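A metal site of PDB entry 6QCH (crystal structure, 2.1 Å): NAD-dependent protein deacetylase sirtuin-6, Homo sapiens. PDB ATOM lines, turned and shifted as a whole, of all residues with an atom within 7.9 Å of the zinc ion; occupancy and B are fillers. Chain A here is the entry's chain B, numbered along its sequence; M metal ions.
The zinc ion is bound by the side-chain sulfur (SG) of Cys 138, the side-chain sulfur (SG) of Cys 135, the side-chain sulfur (SG) of Cys 160 and the side-chain sulfur (SG) of Cys 171.
The side-chain sulfur of Cys 138 lies close to the side-chain hydroxyl of Thr 140 (3.2 Å). The backbone NH of Val 162 lies close to the side-chain sulfur of Cys 160. SG of Cys 135 sits close to N of Lys 137, 3.3 Å away. The backbone NH (N) of Cys 135 lies within hydrogen-bond range of the backbone carbonyl oxygen (O) of Thr 140 (3.0 Å). OH of Tyr 142 sits close to SG of Cys 160, 3.2 Å away. SG of Cys 171 lies close to N of Gly 173, at 3.7 Å. O of Gly 173 lies close to SG of Cys 135, at 3.8 Å. The backbone NH of Cys 160 sits at hydrogen-bond distance from the backbone carbonyl oxygen of Gly 173 (2.7 Å).
Four residues have an atom within 4 Å of the zinc ion: Cys 135, Cys 138, Cys 160 and Cys 171. Along chain A the residues within 4 Å of the zinc ion span positions 135 to 171.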
ATOM      1  N   GLU A 134     -22.971   5.206  -9.436  1.00  0.00           N
ATOM      2  CA  GLU A 134     -21.805   5.636 -10.261  1.00  0.00           C
ATOM      3  C   GLU A 134     -21.929   7.133 -10.534  1.00  0.00           C
ATOM      4  O   GLU A 134     -23.064   7.605 -10.781  1.00  0.00           O
ATOM      5  CB  GLU A 134     -21.799   4.812 -11.546  1.00  0.00           C
ATOM      6  CG  GLU A 134     -20.652   5.110 -12.501  1.00  0.00           C
ATOM      7  CD  GLU A 134     -20.763   4.228 -13.728  1.00  0.00           C
ATOM      8  OE1 GLU A 134     -20.591   3.007 -13.581  1.00  0.00           O
ATOM      9  OE2 GLU A 134     -21.089   4.768 -14.817  1.00  0.00           O
ATOM     10  N   CYS A 135     -20.820   7.854 -10.485  1.00  0.00           N
ATOM     11  CA  CYS A 135     -20.782   9.302 -10.825  1.00  0.00           C
ATOM     12  C   CYS A 135     -20.915   9.492 -12.337  1.00  0.00           C
ATOM     13  O   CYS A 135     -20.100   8.925 -13.104  1.00  0.00           O
ATOM     14  CB  CYS A 135     -19.495   9.980 -10.370  1.00  0.00           C
ATOM     15  SG  CYS A 135     -19.512  11.751 -10.766  1.00  0.00           S
ATOM     16  N   ALA A 136     -21.848  10.354 -12.721  1.00  0.00           N
ATOM     17  CA  ALA A 136     -22.141  10.667 -14.126  1.00  0.00           C
ATOM     18  C   ALA A 136     -20.901  11.279 -14.778  1.00  0.00           C
ATOM     19  O   ALA A 136     -20.703  11.038 -15.976  1.00  0.00           O
ATOM     20  CB  ALA A 136     -23.314  11.594 -14.175  1.00  0.00           C
ATOM     21  N   LYS A 137     -20.079  11.992 -14.009  1.00  0.00           N
ATOM     22  CA  LYS A 137     -18.911  12.673 -14.623  1.00  0.00           C
ATOM     23  C   LYS A 137     -17.621  11.856 -14.592  1.00  0.00           C
ATOM     24  O   LYS A 137     -17.217  11.447 -15.674  1.00  0.00           O
ATOM     25  CB  LYS A 137     -18.684  14.007 -13.929  1.00  0.00           C
ATOM     26  CG  LYS A 137     -19.899  14.897 -13.871  1.00  0.00           C
ATOM     27  CD  LYS A 137     -19.517  16.312 -13.602  1.00  0.00           C
ATOM     28  CE  LYS A 137     -20.620  17.148 -13.015  1.00  0.00           C
ATOM     29  NZ  LYS A 137     -20.097  18.379 -12.398  1.00  0.00           N
ATOM     30  N   CYS A 138     -17.028  11.612 -13.418  1.00  0.00           N
ATOM     31  CA  CYS A 138     -15.714  10.922 -13.307  1.00  0.00           C
ATOM     32  C   CYS A 138     -15.851   9.393 -13.310  1.00  0.00           C
ATOM     33  O   CYS A 138     -14.809   8.736 -13.396  1.00  0.00           O
ATOM     34  CB  CYS A 138     -14.944  11.367 -12.072  1.00  0.00           C
ATOM     35  SG  CYS A 138     -15.749  10.909 -10.515  1.00  0.00           S
ATOM     36  N   LYS A 139     -17.078   8.831 -13.236  1.00  0.00           N
ATOM     37  CA  LYS A 139     -17.377   7.375 -13.396  1.00  0.00           C
ATOM     38  C   LYS A 139     -16.875   6.558 -12.190  1.00  0.00           C
ATOM     39  O   LYS A 139     -16.734   5.311 -12.322  1.00  0.00           O
ATOM     40  CB  LYS A 139     -16.768   6.859 -14.703  1.00  0.00           C
ATOM     41  CG  LYS A 139     -17.059   7.723 -15.937  1.00  0.00           C
ATOM     42  CD  LYS A 139     -18.484   7.610 -16.436  1.00  0.00           C
ATOM     43  CE  LYS A 139     -18.761   6.280 -17.104  1.00  0.00           C
ATOM     44  NZ  LYS A 139     -19.576   6.434 -18.328  1.00  0.00           N
ATOM     45  N   THR A 140     -16.619   7.235 -11.059  1.00  0.00           N
ATOM     46  CA  THR A 140     -16.272   6.651  -9.734  1.00  0.00           C
ATOM     47  C   THR A 140     -17.498   5.937  -9.167  1.00  0.00           C
ATOM     48  O   THR A 140     -18.544   6.596  -8.994  1.00  0.00           O
ATOM     49  CB  THR A 140     -15.778   7.731  -8.763  1.00  0.00           C
ATOM     50  OG1 THR A 140     -14.546   8.242  -9.261  1.00  0.00           O
ATOM     51  CG2 THR A 140     -15.567   7.224  -7.355  1.00  0.00           C
ATOM     52  N   GLN A 141     -17.364   4.643  -8.867  1.00  0.00           N
ATOM     53  CA  GLN A 141     -18.438   3.791  -8.296  1.00  0.00           C
ATOM     54  C   GLN A 141     -18.358   3.848  -6.778  1.00  0.00           C
ATOM     55  O   GLN A 141     -17.243   3.912  -6.241  1.00  0.00           O
ATOM     56  CB  GLN A 141     -18.305   2.350  -8.798  1.00  0.00           C
ATOM     57  CG  GLN A 141     -17.904   2.302 -10.261  1.00  0.00           C
ATOM     58  CD  GLN A 141     -18.518   1.141 -10.988  1.00  0.00           C
ATOM     59  OE1 GLN A 141     -18.012   0.024 -10.962  1.00  0.00           O
ATOM     60  NE2 GLN A 141     -19.625   1.404 -11.657  1.00  0.00           N
ATOM     61  N   TYR A 142     -19.522   3.817  -6.125  1.00  0.00           N
ATOM     62  CA  TYR A 142     -19.677   3.786  -4.651  1.00  0.00           C
ATOM     63  C   TYR A 142     -20.410   2.491  -4.277  1.00  0.00           C
ATOM     64  O   TYR A 142     -21.566   2.354  -4.712  1.00  0.00           O
ATOM     65  CB  TYR A 142     -20.445   5.035  -4.207  1.00  0.00           C
ATOM     66  CG  TYR A 142     -19.707   6.314  -4.475  1.00  0.00           C
ATOM     67  CD1 TYR A 142     -19.723   6.922  -5.728  1.00  0.00           C
ATOM     68  CD2 TYR A 142     -18.958   6.920  -3.488  1.00  0.00           C
ATOM     69  CE1 TYR A 142     -19.032   8.089  -5.980  1.00  0.00           C
ATOM     70  CE2 TYR A 142     -18.268   8.094  -3.713  1.00  0.00           C
ATOM     71  CZ  TYR A 142     -18.286   8.677  -4.968  1.00  0.00           C
ATOM     72  OH  TYR A 142     -17.595   9.834  -5.189  1.00  0.00           O
ATOM     73  N   LEU A 159     -24.428  13.424  -4.712  1.00  0.00           N
ATOM     74  CA  LEU A 159     -23.308  13.886  -5.568  1.00  0.00           C
ATOM     75  C   LEU A 159     -21.988  13.176  -5.190  1.00  0.00           C
ATOM     76  O   LEU A 159     -21.768  12.882  -4.012  1.00  0.00           O
ATOM     77  CB  LEU A 159     -23.205  15.414  -5.458  1.00  0.00           C
ATOM     78  CG  LEU A 159     -24.520  16.182  -5.566  1.00  0.00           C
ATOM     79  CD1 LEU A 159     -24.274  17.682  -5.484  1.00  0.00           C
ATOM     80  CD2 LEU A 159     -25.295  15.835  -6.838  1.00  0.00           C
ATOM     81  N   CYS A 160     -21.138  12.922  -6.194  1.00  0.00           N
ATOM     82  CA  CYS A 160     -19.730  12.486  -6.085  1.00  0.00           C
ATOM     83  C   CYS A 160     -18.963  13.391  -5.117  1.00  0.00           C
ATOM     84  O   CYS A 160     -19.281  14.578  -5.046  1.00  0.00           O
ATOM     85  CB  CYS A 160     -19.052  12.519  -7.449  1.00  0.00           C
ATOM     86  SG  CYS A 160     -17.276  12.138  -7.419  1.00  0.00           S
ATOM     87  N   THR A 161     -17.979  12.815  -4.418  1.00  0.00           N
ATOM     88  CA  THR A 161     -17.140  13.466  -3.386  1.00  0.00           C
ATOM     89  C   THR A 161     -15.645  13.301  -3.735  1.00  0.00           C
ATOM     90  O   THR A 161     -14.822  13.688  -2.890  1.00  0.00           O
ATOM     91  CB  THR A 161     -17.514  12.900  -2.012  1.00  0.00           C
ATOM     92  OG1 THR A 161     -17.262  11.492  -1.999  1.00  0.00           O
ATOM     93  CG2 THR A 161     -18.956  13.164  -1.632  1.00  0.00           C
ATOM     94  N   VAL A 162     -15.304  12.822  -4.949  1.00  0.00           N
ATOM     95  CA  VAL A 162     -13.893  12.508  -5.384  1.00  0.00           C
ATOM     96  C   VAL A 162     -12.966  13.690  -5.044  1.00  0.00           C
ATOM     97  O   VAL A 162     -13.355  14.850  -5.299  1.00  0.00           O
ATOM     98  CB  VAL A 162     -13.802  12.148  -6.887  1.00  0.00           C
ATOM     99  CG1 VAL A 162     -12.397  12.330  -7.459  1.00  0.00           C
ATOM    100  CG2 VAL A 162     -14.290  10.729  -7.176  1.00  0.00           C
ATOM    101  N   CYS A 171     -15.624  17.366  -7.072  1.00  0.00           N
ATOM    102  CA  CYS A 171     -16.146  16.859  -8.374  1.00  0.00           C
ATOM    103  C   CYS A 171     -17.656  17.033  -8.464  1.00  0.00           C
ATOM    104  O   CYS A 171     -18.144  17.315  -9.575  1.00  0.00           O
ATOM    105  CB  CYS A 171     -15.819  15.386  -8.581  1.00  0.00           C
ATOM    106  SG  CYS A 171     -16.724  14.665  -9.971  1.00  0.00           S
ATOM    107  N   ARG A 172     -18.371  16.748  -7.378  1.00  0.00           N
ATOM    108  CA  ARG A 172     -19.810  17.092  -7.192  1.00  0.00           C
ATOM    109  C   ARG A 172     -20.677  16.555  -8.338  1.00  0.00           C
ATOM    110  O   ARG A 172     -21.863  16.958  -8.413  1.00  0.00           O
ATOM    111  CB  ARG A 172     -19.916  18.614  -7.056  1.00  0.00           C
ATOM    112  CG  ARG A 172     -18.954  19.209  -6.040  1.00  0.00           C
ATOM    113  CD  ARG A 172     -19.399  20.583  -5.598  1.00  0.00           C
ATOM    114  NE  ARG A 172     -20.786  20.514  -5.132  1.00  0.00           N
ATOM    115  CZ  ARG A 172     -21.654  21.509  -5.136  1.00  0.00           C
ATOM    116  NH1 ARG A 172     -21.318  22.714  -5.576  1.00  0.00           N
ATOM    117  NH2 ARG A 172     -22.883  21.299  -4.700  1.00  0.00           N
ATOM    118  N   GLY A 173     -20.152  15.655  -9.183  1.00  0.00           N
ATOM    119  CA  GLY A 173     -20.898  15.003 -10.267  1.00  0.00           C
ATOM    120  C   GLY A 173     -22.106  14.229  -9.736  1.00  0.00           C
ATOM    121  O   GLY A 173     -21.984  13.650  -8.636  1.00  0.00           O
ATOM    122  N   GLU A 174     -23.219  14.259 -10.483  1.00  0.00           N
ATOM    123  CA  GLU A 174     -24.495  13.512 -10.246  1.00  0.00           C
ATOM    124  C   GLU A 174     -24.216  12.004 -10.135  1.00  0.00           C
ATOM    125  O   GLU A 174     -23.539  11.466 -11.070  1.00  0.00           O
ATOM    126  CB  GLU A 174     -25.440  13.820 -11.418  1.00  0.00           C
ATOM    127  CG  GLU A 174     -26.832  13.190 -11.316  1.00  0.00           C
ATOM    128  CD  GLU A 174     -27.664  13.219 -12.592  1.00  0.00           C
ATOM    129  OE1 GLU A 174     -28.600  14.054 -12.679  1.00  0.00           O
ATOM    130  OE2 GLU A 174     -27.407  12.384 -13.503  1.00  0.00           O
ATOM    131  N   LEU A 175     -24.716  11.339  -9.080  1.00  0.00           N
ATOM    132  CA  LEU A 175     -24.616   9.864  -8.856  1.00  0.00           C
ATOM    133  C   LEU A 175     -25.921   9.210  -9.333  1.00  0.00           C
ATOM    134  O   LEU A 175     -27.010   9.707  -8.958  1.00  0.00           O
ATOM    135  CB  LEU A 175     -24.362   9.529  -7.383  1.00  0.00           C
ATOM    136  CG  LEU A 175     -23.124  10.148  -6.735  1.00  0.00           C
ATOM    137  CD1 LEU A 175     -23.025   9.751  -5.264  1.00  0.00           C
ATOM    138  CD2 LEU A 175     -21.842   9.727  -7.444  1.00  0.00           C
HETATM  139 ZN    ZN M   1     -17.444  12.132 -10.015  1.00  0.00          ZN
